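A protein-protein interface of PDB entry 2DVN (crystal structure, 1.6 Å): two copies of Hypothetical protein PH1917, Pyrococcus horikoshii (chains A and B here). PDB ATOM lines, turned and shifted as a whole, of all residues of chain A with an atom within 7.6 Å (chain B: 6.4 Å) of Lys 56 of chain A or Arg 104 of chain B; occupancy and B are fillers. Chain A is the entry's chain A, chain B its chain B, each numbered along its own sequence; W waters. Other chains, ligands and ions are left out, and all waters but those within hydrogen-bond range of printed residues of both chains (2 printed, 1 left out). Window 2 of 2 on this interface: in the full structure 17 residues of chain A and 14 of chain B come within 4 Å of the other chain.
Among the printed residues, pairs that only touch across the chains: Pro 58 of chain A with Glu 71 of chain B (3.3 Å), Phe 4 of chain A with Trp 127 of chain B (3.5 Å), Leu 30 of chain A with Trp 127 of chain B (3.5 Å), Pro 58 of chain A with Arg 104 of chain B (3.6 Å), Pro 58 of chain A with Trp 127 of chain B (3.6 Å), Val 57 of chain A with Arg 104 of chain B (3.8 Å) and Phe 4 of chain A with Tyr 106 of chain B (3.9 Å).
Hydrophobic or aromatic side chains of chain A that line the printed part of chain B: Phe 4, Leu 30 and Pro 58. Among the printed residues, no Asp or Glu carboxylate lies within 4 Å of a Lys or Arg side-chain nitrogen of the other chain.
Printed residues of chain B within 4 Å of Phe 4 of chain A: Tyr 106 (3.9 Å) and Trp 127 (3.5 Å). Of the printed residues of chain B, Leu 30 of chain A touches Trp 127. Of chain B, only Arg 104 (3.3 Å) comes within 4 Å of Lys 56 of chain A. Of the printed residues of chain B, Val 57 of chain A touches Arg 104 (3.8 Å). Printed residues of chain A within 4 Å of Glu 71 of chain B: Pro 58 (3.3 Å). Of the printed residues of chain A, Arg 104 of chain B touches Lys 56 (3.3 Å), Val 57 (3.8 Å) and Pro 58 (3.6 Å). Of the printed residues of chain A, Tyr 106 of chain B touches Phe 4 (3.9 Å). The nearest residue of chain B that does not touch Lys 56 of chain A is Glu 149 of chain B (6.3 Å). The nearest residue of chain A that does not touch Arg 104 of chain B is Gly 55 of chain A (5.6 Å). The nearest printed residue of chain A that does not touch Tyr 106 of chain B is Pro 58 of chain A (6.6 Å).
O of Trp 52 of chain A sits at hydrogen-bond distance from NZ of Lys 56 of chain A (3.0 Å). The backbone carbonyl oxygen of Tyr 106 of chain B is in hydrogen-bond range of the backbone NH of Phe 69 of chain B, 2.8 Å away. The side-chain carboxylate (OD2) of Asp 102 of chain B sits close to the side-chain carboxylate (OE2) of Glu 71 of chain B, at 2.7 Å. OE1 of Glu 71 of chain B lies within salt-bridge range of NE of Arg 104 of chain B. OD1 of Asp 102 of chain B sits at hydrogen-bond distance from N of Arg 104 of chain B, 3.1 Å away. O of Trp 127 of chain B sits at hydrogen-bond distance from N of Glu 149 of chain B, at 2.9 Å.
Water W2 lies within hydrogen-bond range of O of Gly 55 of chain A (2.9 Å) and NH1 of Arg 104 of chain B (3.0 Å). Water W1 lies within hydrogen-bond range of O of Val 57 of chain A (3.0 Å) and NH2 of Arg 104 of chain B (3.1 Å).
No position is printed for both chains.
O of Lys 56 of chain A sits at hydrogen-bond distance from NH1 of Arg 104 of chain B (3.3 Å).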
ATOM      1  N   PHE A   4      -5.549  14.720   9.087  1.00  0.00           N
ATOM      2  CA  PHE A   4      -6.853  14.287   8.611  1.00  0.00           C
ATOM      3  C   PHE A   4      -7.692  15.525   8.346  1.00  0.00           C
ATOM      4  O   PHE A   4      -7.913  16.343   9.236  1.00  0.00           O
ATOM      5  CB  PHE A   4      -7.512  13.377   9.644  1.00  0.00           C
ATOM      6  CG  PHE A   4      -6.696  12.161   9.955  1.00  0.00           C
ATOM      7  CD1 PHE A   4      -5.909  12.102  11.104  1.00  0.00           C
ATOM      8  CD2 PHE A   4      -6.651  11.102   9.053  1.00  0.00           C
ATOM      9  CE1 PHE A   4      -5.086  11.004  11.347  1.00  0.00           C
ATOM     10  CE2 PHE A   4      -5.832  10.005   9.287  1.00  0.00           C
ATOM     11  CZ  PHE A   4      -5.048   9.957  10.435  1.00  0.00           C
ATOM     12  N   ILE A   6     -11.169  16.879   7.590  1.00  0.00           N
ATOM     13  CA  ILE A   6     -12.598  16.572   7.661  1.00  0.00           C
ATOM     14  C   ILE A   6     -13.312  17.541   6.722  1.00  0.00           C
ATOM     15  O   ILE A   6     -13.459  18.729   7.029  1.00  0.00           O
ATOM     16  CB  ILE A   6     -13.150  16.772   9.089  1.00  0.00           C
ATOM     17  CG1 ILE A   6     -12.209  16.137  10.123  1.00  0.00           C
ATOM     18  CG2 ILE A   6     -14.565  16.208   9.175  1.00  0.00           C
ATOM     19  CD1 ILE A   6     -11.880  14.686   9.880  1.00  0.00           C
ATOM     20  N   LEU A  30     -11.405  12.896   5.145  1.00  0.00           N
ATOM     21  CA  LEU A  30     -12.354  12.128   5.936  1.00  0.00           C
ATOM     22  C   LEU A  30     -13.693  12.854   5.870  1.00  0.00           C
ATOM     23  O   LEU A  30     -13.833  13.959   6.397  1.00  0.00           O
ATOM     24  CB  LEU A  30     -11.876  12.043   7.394  1.00  0.00           C
ATOM     25  CG  LEU A  30     -12.559  11.076   8.371  1.00  0.00           C
ATOM     26  CD1 LEU A  30     -11.930  11.226   9.755  1.00  0.00           C
ATOM     27  CD2 LEU A  30     -14.043  11.355   8.443  1.00  0.00           C
ATOM     28  N   HIS A  32     -17.060  13.589   7.189  1.00  0.00           N
ATOM     29  CA  HIS A  32     -17.791  13.435   8.439  1.00  0.00           C
ATOM     30  C   HIS A  32     -18.520  14.747   8.677  1.00  0.00           C
ATOM     31  O   HIS A  32     -17.980  15.672   9.287  1.00  0.00           O
ATOM     32  CB  HIS A  32     -16.829  13.147   9.597  1.00  0.00           C
ATOM     33  CG  HIS A  32     -17.512  12.777  10.876  1.00  0.00           C
ATOM     34  ND1 HIS A  32     -18.397  13.614  11.520  1.00  0.00           N
ATOM     35  CD2 HIS A  32     -17.440  11.655  11.632  1.00  0.00           C
ATOM     36  CE1 HIS A  32     -18.836  13.025  12.617  1.00  0.00           C
ATOM     37  NE2 HIS A  32     -18.271  11.836  12.709  1.00  0.00           N
ATOM     38  N   GLU A  33     -19.745  14.828   8.172  1.00  0.00           N
ATOM     39  CA  GLU A  33     -20.537  16.039   8.316  1.00  0.00           C
ATOM     40  C   GLU A  33     -20.588  16.492   9.765  1.00  0.00           C
ATOM     41  O   GLU A  33     -20.773  15.688  10.677  1.00  0.00           O
ATOM     42  CB  GLU A  33     -21.960  15.809   7.797  1.00  0.00           C
ATOM     43  CG  GLU A  33     -22.045  15.520   6.302  1.00  0.00           C
ATOM     44  CD  GLU A  33     -21.681  16.719   5.443  1.00  0.00           C
ATOM     45  OE1 GLU A  33     -21.651  16.574   4.201  1.00  0.00           O
ATOM     46  OE2 GLU A  33     -21.430  17.806   6.005  1.00  0.00           O
ATOM     47  N   PRO A  35     -21.982  19.922  12.380  1.00  0.00           N
ATOM     48  CA  PRO A  35     -22.893  21.064  12.389  1.00  0.00           C
ATOM     49  C   PRO A  35     -22.150  22.350  12.059  1.00  0.00           C
ATOM     50  O   PRO A  35     -21.087  22.621  12.614  1.00  0.00           O
ATOM     51  CB  PRO A  35     -23.433  21.070  13.819  1.00  0.00           C
ATOM     52  CG  PRO A  35     -23.297  19.629  14.250  1.00  0.00           C
ATOM     53  CD  PRO A  35     -21.955  19.256  13.691  1.00  0.00           C
ATOM     54  N   GLY A  49     -17.335  23.756  15.096  1.00  0.00           N
ATOM     55  CA  GLY A  49     -17.023  22.525  14.388  1.00  0.00           C
ATOM     56  C   GLY A  49     -15.944  21.709  15.072  1.00  0.00           C
ATOM     57  O   GLY A  49     -16.076  20.493  15.221  1.00  0.00           O
ATOM     58  N   ILE A  50     -14.865  22.368  15.486  1.00  0.00           N
ATOM     59  CA  ILE A  50     -13.800  21.635  16.162  1.00  0.00           C
ATOM     60  C   ILE A  50     -14.275  21.050  17.492  1.00  0.00           C
ATOM     61  O   ILE A  50     -13.983  19.915  17.850  1.00  0.00           O
ATOM     62  CB  ILE A  50     -12.660  22.618  16.426  1.00  0.00           C
ATOM     63  CG1 ILE A  50     -11.955  22.979  15.116  1.00  0.00           C
ATOM     64  CG2 ILE A  50     -11.613  21.969  17.353  1.00  0.00           C
ATOM     65  CD1 ILE A  50     -10.837  24.003  15.325  1.00  0.00           C
ATOM     66  N   SER A  51     -14.986  21.893  18.263  1.00  0.00           N
ATOM     67  CA  SER A  51     -15.498  21.443  19.552  1.00  0.00           C
ATOM     68  C   SER A  51     -16.409  20.220  19.402  1.00  0.00           C
ATOM     69  O   SER A  51     -16.497  19.355  20.260  1.00  0.00           O
ATOM     70  CB  SER A  51     -16.280  22.596  20.181  1.00  0.00           C
ATOM     71  OG  SER A  51     -15.389  23.677  20.456  1.00  0.00           O
ATOM     72  N   TRP A  52     -17.136  20.195  18.269  1.00  0.00           N
ATOM     73  CA  TRP A  52     -18.069  19.102  18.009  1.00  0.00           C
ATOM     74  C   TRP A  52     -17.343  17.822  17.583  1.00  0.00           C
ATOM     75  O   TRP A  52     -17.729  16.713  17.930  1.00  0.00           O
ATOM     76  CB  TRP A  52     -19.029  19.548  16.905  1.00  0.00           C
ATOM     77  CG  TRP A  52     -19.960  18.449  16.560  1.00  0.00           C
ATOM     78  CD1 TRP A  52     -19.756  17.443  15.589  1.00  0.00           C
ATOM     79  CD2 TRP A  52     -21.260  18.202  17.145  1.00  0.00           C
ATOM     80  NE1 TRP A  52     -20.804  16.581  15.508  1.00  0.00           N
ATOM     81  CE2 TRP A  52     -21.796  17.056  16.505  1.00  0.00           C
ATOM     82  CE3 TRP A  52     -22.005  18.844  18.130  1.00  0.00           C
ATOM     83  CZ2 TRP A  52     -23.045  16.580  16.868  1.00  0.00           C
ATOM     84  CZ3 TRP A  52     -23.255  18.369  18.493  1.00  0.00           C
ATOM     85  CH2 TRP A  52     -23.779  17.232  17.854  1.00  0.00           C
ATOM     86  N   LEU A  53     -16.290  18.022  16.766  1.00  0.00           N
ATOM     87  CA  LEU A  53     -15.635  16.875  16.146  1.00  0.00           C
ATOM     88  C   LEU A  53     -14.678  16.154  17.101  1.00  0.00           C
ATOM     89  O   LEU A  53     -14.474  14.949  17.035  1.00  0.00           O
ATOM     90  CB  LEU A  53     -14.870  17.364  14.914  1.00  0.00           C
ATOM     91  CG  LEU A  53     -15.784  17.603  13.711  1.00  0.00           C
ATOM     92  CD1 LEU A  53     -15.063  18.306  12.561  1.00  0.00           C
ATOM     93  CD2 LEU A  53     -16.355  16.309  13.128  1.00  0.00           C
ATOM     94  N   LYS A  54     -14.045  16.939  17.991  1.00  0.00           N
ATOM     95  CA  LYS A  54     -13.032  16.331  18.849  1.00  0.00           C
ATOM     96  C   LYS A  54     -13.559  15.099  19.588  1.00  0.00           C
ATOM     97  O   LYS A  54     -14.654  15.094  20.133  1.00  0.00           O
ATOM     98  CB  LYS A  54     -12.462  17.375  19.818  1.00  0.00           C
ATOM     99  CG  LYS A  54     -13.484  17.956  20.801  1.00  0.00           C
ATOM    100  CD  LYS A  54     -12.859  19.050  21.676  1.00  0.00           C
ATOM    101  CE  LYS A  54     -13.826  19.607  22.727  1.00  0.00           C
ATOM    102  NZ  LYS A  54     -13.158  20.651  23.512  1.00  0.00           N
ATOM    103  N   GLY A  55     -12.755  14.041  19.532  1.00  0.00           N
ATOM    104  CA  GLY A  55     -13.127  12.779  20.144  1.00  0.00           C
ATOM    105  C   GLY A  55     -13.893  11.853  19.214  1.00  0.00           C
ATOM    106  O   GLY A  55     -14.102  10.681  19.533  1.00  0.00           O
ATOM    107  N   LYS A  56     -14.305  12.365  18.059  1.00  0.00           N
ATOM    108  CA  LYS A  56     -15.065  11.566  17.102  1.00  0.00           C
ATOM    109  C   LYS A  56     -14.265  11.238  15.847  1.00  0.00           C
ATOM    110  O   LYS A  56     -14.672  10.394  15.045  1.00  0.00           O
ATOM    111  CB  LYS A  56     -16.337  12.311  16.705  1.00  0.00           C
ATOM    112  CG  LYS A  56     -17.200  12.700  17.889  1.00  0.00           C
ATOM    113  CD  LYS A  56     -18.355  13.588  17.472  1.00  0.00           C
ATOM    114  CE  LYS A  56     -19.145  14.050  18.690  1.00  0.00           C
ATOM    115  NZ  LYS A  56     -20.165  15.073  18.340  1.00  0.00           N
ATOM    116  N   VAL A  57     -13.136  11.916  15.678  1.00  0.00           N
ATOM    117  CA  VAL A  57     -12.283  11.707  14.515  1.00  0.00           C
ATOM    118  C   VAL A  57     -10.812  11.599  14.910  1.00  0.00           C
ATOM    119  O   VAL A  57     -10.405  12.048  15.983  1.00  0.00           O
ATOM    120  CB  VAL A  57     -12.439  12.867  13.503  1.00  0.00           C
ATOM    121  CG1 VAL A  57     -13.865  12.915  12.979  1.00  0.00           C
ATOM    122  CG2 VAL A  57     -12.077  14.190  14.167  1.00  0.00           C
ATOM    123  N   PRO A  58      -9.991  10.988  14.044  1.00  0.00           N
ATOM    124  CA  PRO A  58      -8.562  10.833  14.316  1.00  0.00           C
ATOM    125  C   PRO A  58      -7.846  12.179  14.351  1.00  0.00           C
ATOM    126  O   PRO A  58      -8.308  13.155  13.756  1.00  0.00           O
ATOM    127  CB  PRO A  58      -8.091   9.930  13.172  1.00  0.00           C
ATOM    128  CG  PRO A  58      -9.045  10.243  12.076  1.00  0.00           C
ATOM    129  CD  PRO A  58     -10.362  10.310  12.792  1.00  0.00           C
ATOM    130  N   GLU A  59      -6.725  12.219  15.062  1.00  0.00           N
ATOM    131  CA  GLU A  59      -5.929  13.431  15.213  1.00  0.00           C
ATOM    132  C   GLU A  59      -4.520  13.255  14.647  1.00  0.00           C
ATOM    133  O   GLU A  59      -4.006  12.140  14.572  1.00  0.00           O
ATOM    134  CB  GLU A  59      -5.845  13.801  16.696  1.00  0.00           C
ATOM    135  CG  GLU A  59      -7.177  14.209  17.304  1.00  0.00           C
ATOM    136  CD  GLU A  59      -7.192  14.099  18.821  1.00  0.00           C
ATOM    137  OE1 GLU A  59      -6.152  14.374  19.452  1.00  0.00           O
ATOM    138  OE2 GLU A  59      -8.253  13.747  19.379  1.00  0.00           O
ATOM    139  N   PHE A  61      -6.388  16.763  13.241  1.00  0.00           N
ATOM    140  CA  PHE A  61      -7.321  16.989  12.151  1.00  0.00           C
ATOM    141  C   PHE A  61      -7.512  18.462  11.860  1.00  0.00           C
ATOM    142  O   PHE A  61      -7.174  19.324  12.673  1.00  0.00           O
ATOM    143  CB  PHE A  61      -8.676  16.307  12.438  1.00  0.00           C
ATOM    144  CG  PHE A  61      -9.501  16.962  13.520  1.00  0.00           C
ATOM    145  CD1 PHE A  61     -10.303  18.064  13.236  1.00  0.00           C
ATOM    146  CD2 PHE A  61      -9.528  16.434  14.808  1.00  0.00           C
ATOM    147  CE1 PHE A  61     -11.126  18.626  14.215  1.00  0.00           C
ATOM    148  CE2 PHE A  61     -10.346  16.988  15.794  1.00  0.00           C
ATOM    149  CZ  PHE A  61     -11.147  18.085  15.497  1.00  0.00           C
ATOM    150  N   PHE B  69      -4.677   1.271   6.038  1.00  0.00           N
ATOM    151  CA  PHE B  69      -3.955   1.943   7.114  1.00  0.00           C
ATOM    152  C   PHE B  69      -4.754   1.824   8.407  1.00  0.00           C
ATOM    153  O   PHE B  69      -5.825   2.420   8.542  1.00  0.00           O
ATOM    154  CB  PHE B  69      -3.752   3.417   6.736  1.00  0.00           C
ATOM    155  CG  PHE B  69      -2.919   3.614   5.497  1.00  0.00           C
ATOM    156  CD1 PHE B  69      -1.569   3.940   5.595  1.00  0.00           C
ATOM    157  CD2 PHE B  69      -3.474   3.433   4.231  1.00  0.00           C
ATOM    158  CE1 PHE B  69      -0.782   4.080   4.453  1.00  0.00           C
ATOM    159  CE2 PHE B  69      -2.693   3.570   3.079  1.00  0.00           C
ATOM    160  CZ  PHE B  69      -1.342   3.894   3.195  1.00  0.00           C
ATOM    161  N   ILE B  70      -4.224   1.056   9.356  1.00  0.00           N
ATOM    162  CA  ILE B  70      -4.892   0.837  10.641  1.00  0.00           C
ATOM    163  C   ILE B  70      -4.379   1.774  11.748  1.00  0.00           C
ATOM    164  O   ILE B  70      -3.204   1.810  12.091  1.00  0.00           O
ATOM    165  CB  ILE B  70      -4.696  -0.630  11.031  1.00  0.00           C
ATOM    166  CG1 ILE B  70      -5.252  -1.537   9.927  1.00  0.00           C
ATOM    167  CG2 ILE B  70      -5.476  -0.935  12.326  1.00  0.00           C
ATOM    168  CD1 ILE B  70      -4.948  -3.017  10.172  1.00  0.00           C
ATOM    169  N   GLU B  71      -5.330   2.573  12.288  1.00  0.00           N
ATOM    170  CA  GLU B  71      -5.010   3.609  13.274  1.00  0.00           C
ATOM    171  C   GLU B  71      -4.165   3.091  14.447  1.00  0.00           C
ATOM    172  O   GLU B  71      -3.132   3.647  14.804  1.00  0.00           O
ATOM    173  CB  GLU B  71      -6.341   4.165  13.798  1.00  0.00           C
ATOM    174  CG  GLU B  71      -6.186   5.439  14.633  1.00  0.00           C
ATOM    175  CD  GLU B  71      -7.495   6.200  14.640  1.00  0.00           C
ATOM    176  OE1 GLU B  71      -7.941   6.609  13.577  1.00  0.00           O
ATOM    177  OE2 GLU B  71      -8.058   6.387  15.718  1.00  0.00           O
ATOM    178  N   SER B  72      -4.664   2.013  15.079  1.00  0.00           N
ATOM    179  CA  SER B  72      -4.003   1.509  16.284  1.00  0.00           C
ATOM    180  C   SER B  72      -2.628   0.888  15.988  1.00  0.00           C
ATOM    181  O   SER B  72      -1.853   0.578  16.882  1.00  0.00           O
ATOM    182  CB  SER B  72      -4.917   0.465  16.928  1.00  0.00           C
ATOM    183  OG  SER B  72      -5.959   1.127  17.644  1.00  0.00           O
ATOM    184  N   MET B  97      -4.478  -6.825  16.612  1.00  0.00           N
ATOM    185  CA  MET B  97      -5.588  -6.004  17.075  1.00  0.00           C
ATOM    186  C   MET B  97      -6.316  -6.547  18.299  1.00  0.00           C
ATOM    187  O   MET B  97      -7.267  -5.933  18.780  1.00  0.00           O
ATOM    188  CB  MET B  97      -6.592  -5.806  15.936  1.00  0.00           C
ATOM    189  CG  MET B  97      -6.055  -4.970  14.786  1.00  0.00           C
ATOM    190  SD  MET B  97      -5.659  -3.292  15.307  1.00  0.00           S
ATOM    191  CE  MET B  97      -7.298  -2.555  15.299  1.00  0.00           C
ATOM    192  N   GLU B 101      -9.457  -1.352  21.374  1.00  0.00           N
ATOM    193  CA  GLU B 101     -10.787  -0.756  21.398  1.00  0.00           C
ATOM    194  C   GLU B 101     -10.946   0.107  20.144  1.00  0.00           C
ATOM    195  O   GLU B 101     -12.001   0.160  19.525  1.00  0.00           O
ATOM    196  CB  GLU B 101     -10.965   0.087  22.661  1.00  0.00           C
ATOM    197  CG  GLU B 101     -12.402   0.176  23.133  1.00  0.00           C
ATOM    198  CD  GLU B 101     -12.927  -1.167  23.605  1.00  0.00           C
ATOM    199  OE1 GLU B 101     -12.378  -1.702  24.592  1.00  0.00           O
ATOM    200  OE2 GLU B 101     -13.883  -1.688  22.990  1.00  0.00           O
ATOM    201  N   ASP B 102      -9.825   0.775  19.820  1.00  0.00           N
ATOM    202  CA  ASP B 102      -9.865   1.625  18.647  1.00  0.00           C
ATOM    203  C   ASP B 102      -9.483   0.779  17.449  1.00  0.00           C
ATOM    204  O   ASP B 102      -8.329   0.429  17.244  1.00  0.00           O
ATOM    205  CB  ASP B 102      -8.790   2.704  18.866  1.00  0.00           C
ATOM    206  CG  ASP B 102      -8.767   3.660  17.682  1.00  0.00           C
ATOM    207  OD1 ASP B 102      -9.410   3.345  16.679  1.00  0.00           O
ATOM    208  OD2 ASP B 102      -8.118   4.698  17.773  1.00  0.00           O
ATOM    209  N   ARG B 103     -10.532   0.448  16.653  1.00  0.00           N
ATOM    210  CA  ARG B 103     -10.332  -0.416  15.495  1.00  0.00           C
ATOM    211  C   ARG B 103     -10.521   0.325  14.176  1.00  0.00           C
ATOM    212  O   ARG B 103     -10.717  -0.284  13.126  1.00  0.00           O
ATOM    213  CB  ARG B 103     -11.283  -1.615  15.584  1.00  0.00           C
ATOM    214  CG  ARG B 103     -11.167  -2.373  16.909  1.00  0.00           C
ATOM    215  CD  ARG B 103     -12.061  -3.602  16.943  1.00  0.00           C
ATOM    216  NE  ARG B 103     -11.543  -4.694  16.126  1.00  0.00           N
ATOM    217  CZ  ARG B 103     -10.543  -5.498  16.490  1.00  0.00           C
ATOM    218  NH1 ARG B 103      -9.946  -5.335  17.662  1.00  0.00           N
ATOM    219  NH2 ARG B 103     -10.150  -6.470  15.681  1.00  0.00           N
ATOM    220  N   ARG B 104     -10.440   1.649  14.238  1.00  0.00           N
ATOM    221  CA  ARG B 104     -10.603   2.477  13.050  1.00  0.00           C
ATOM    222  C   ARG B 104      -9.473   2.242  12.049  1.00  0.00           C
ATOM    223  O   ARG B 104      -8.328   1.980  12.431  1.00  0.00           O
ATOM    224  CB  ARG B 104     -10.654   3.952  13.460  1.00  0.00           C
ATOM    225  CG  ARG B 104     -10.922   4.928  12.325  1.00  0.00           C
ATOM    226  CD  ARG B 104     -11.526   6.216  12.876  1.00  0.00           C
ATOM    227  NE  ARG B 104     -10.746   6.753  13.989  1.00  0.00           N
ATOM    228  CZ  ARG B 104     -11.232   7.575  14.915  1.00  0.00           C
ATOM    229  NH1 ARG B 104     -12.500   7.958  14.865  1.00  0.00           N
ATOM    230  NH2 ARG B 104     -10.457   7.999  15.903  1.00  0.00           N
ATOM    231  N   ALA B 105      -9.811   2.331  10.767  1.00  0.00           N
ATOM    232  CA  ALA B 105      -8.851   2.137   9.689  1.00  0.00           C
ATOM    233  C   ALA B 105      -9.410   2.738   8.407  1.00  0.00           C
ATOM    234  O   ALA B 105     -10.590   3.077   8.331  1.00  0.00           O
ATOM    235  CB  ALA B 105      -8.586   0.643   9.487  1.00  0.00           C
ATOM    236  N   TYR B 106      -8.557   2.883   7.402  1.00  0.00           N
ATOM    237  CA  TYR B 106      -9.011   3.407   6.127  1.00  0.00           C
ATOM    238  C   TYR B 106      -8.208   2.835   4.976  1.00  0.00           C
ATOM    239  O   TYR B 106      -7.036   2.471   5.127  1.00  0.00           O
ATOM    240  CB  TYR B 106      -8.935   4.946   6.097  1.00  0.00           C
ATOM    241  CG  TYR B 106      -7.537   5.537   6.178  1.00  0.00           C
ATOM    242  CD1 TYR B 106      -6.726   5.649   5.043  1.00  0.00           C
ATOM    243  CD2 TYR B 106      -7.025   5.981   7.393  1.00  0.00           C
ATOM    244  CE1 TYR B 106      -5.435   6.191   5.125  1.00  0.00           C
ATOM    245  CE2 TYR B 106      -5.745   6.522   7.488  1.00  0.00           C
ATOM    246  CZ  TYR B 106      -4.954   6.623   6.358  1.00  0.00           C
ATOM    247  OH  TYR B 106      -3.682   7.146   6.474  1.00  0.00           O
ATOM    248  N   TRP B 127     -13.159   5.152   4.833  1.00  0.00           N
ATOM    249  CA  TRP B 127     -12.977   4.861   6.244  1.00  0.00           C
ATOM    250  C   TRP B 127     -13.844   3.707   6.700  1.00  0.00           C
ATOM    251  O   TRP B 127     -14.866   3.404   6.091  1.00  0.00           O
ATOM    252  CB  TRP B 127     -13.289   6.098   7.084  1.00  0.00           C
ATOM    253  CG  TRP B 127     -12.246   7.153   6.962  1.00  0.00           C
ATOM    254  CD1 TRP B 127     -12.117   8.069   5.960  1.00  0.00           C
ATOM    255  CD2 TRP B 127     -11.143   7.364   7.847  1.00  0.00           C
ATOM    256  NE1 TRP B 127     -10.997   8.841   6.166  1.00  0.00           N
ATOM    257  CE2 TRP B 127     -10.380   8.429   7.319  1.00  0.00           C
ATOM    258  CE3 TRP B 127     -10.723   6.755   9.039  1.00  0.00           C
ATOM    259  CZ2 TRP B 127      -9.218   8.899   7.939  1.00  0.00           C
ATOM    260  CZ3 TRP B 127      -9.568   7.221   9.657  1.00  0.00           C
ATOM    261  CH2 TRP B 127      -8.828   8.286   9.106  1.00  0.00           C
ATOM    262  N   GLY B 128     -13.422   3.069   7.784  1.00  0.00           N
ATOM    263  CA  GLY B 128     -14.169   1.951   8.323  1.00  0.00           C
ATOM    264  C   GLY B 128     -13.498   1.465   9.586  1.00  0.00           C
ATOM    265  O   GLY B 128     -12.808   2.230  10.260  1.00  0.00           O
ATOM    266  N   ARG B 129     -13.709   0.197   9.914  1.00  0.00           N
ATOM    267  CA  ARG B 129     -13.098  -0.386  11.098  1.00  0.00           C
ATOM    268  C   ARG B 129     -12.770  -1.849  10.852  1.00  0.00           C
ATOM    269  O   ARG B 129     -13.322  -2.478   9.945  1.00  0.00           O
ATOM    270  CB  ARG B 129     -14.028  -0.262  12.308  1.00  0.00           C
ATOM    271  CG  ARG B 129     -15.325  -1.046  12.208  1.00  0.00           C
ATOM    272  CD  ARG B 129     -16.061  -1.006  13.544  1.00  0.00           C
ATOM    273  NE  ARG B 129     -17.227  -1.885  13.574  1.00  0.00           N
ATOM    274  CZ  ARG B 129     -18.369  -1.641  12.940  1.00  0.00           C
ATOM    275  NH1 ARG B 129     -18.506  -0.537  12.218  1.00  0.00           N
ATOM    276  NH2 ARG B 129     -19.375  -2.501  13.029  1.00  0.00           N
ATOM    277  N   ILE B 130     -11.850  -2.380  11.649  1.00  0.00           N
ATOM    278  CA  ILE B 130     -11.458  -3.774  11.527  1.00  0.00           C
ATOM    279  C   ILE B 130     -12.403  -4.605  12.386  1.00  0.00           C
ATOM    280  O   ILE B 130     -12.632  -4.292  13.557  1.00  0.00           O
ATOM    281  CB  ILE B 130     -10.005  -3.984  12.012  1.00  0.00           C
ATOM    282  CG1 ILE B 130      -9.060  -3.039  11.258  1.00  0.00           C
ATOM    283  CG2 ILE B 130      -9.585  -5.435  11.798  1.00  0.00           C
ATOM    284  CD1 ILE B 130      -9.119  -3.168   9.747  1.00  0.00           C
ATOM    285  N   GLU B 149     -17.439   2.487   6.951  1.00  0.00           N
ATOM    286  CA  GLU B 149     -18.272   3.358   7.765  1.00  0.00           C
ATOM    287  C   GLU B 149     -19.651   3.464   7.125  1.00  0.00           C
ATOM    288  O   GLU B 149     -19.768   3.640   5.912  1.00  0.00           O
ATOM    289  CB  GLU B 149     -17.623   4.740   7.870  1.00  0.00           C
ATOM    290  CG  GLU B 149     -18.364   5.724   8.752  1.00  0.00           C
ATOM    291  CD  GLU B 149     -17.567   6.988   8.977  1.00  0.00           C
ATOM    292  OE1 GLU B 149     -17.147   7.595   7.978  1.00  0.00           O
ATOM    293  OE2 GLU B 149     -17.356   7.378  10.144  1.00  0.00           O
HETATM  294  O   HOH W   1     -10.746  10.036  18.245  1.00  0.00           O
HETATM  295  O   HOH W   2     -12.781   8.792  17.711  1.00  0.00           O
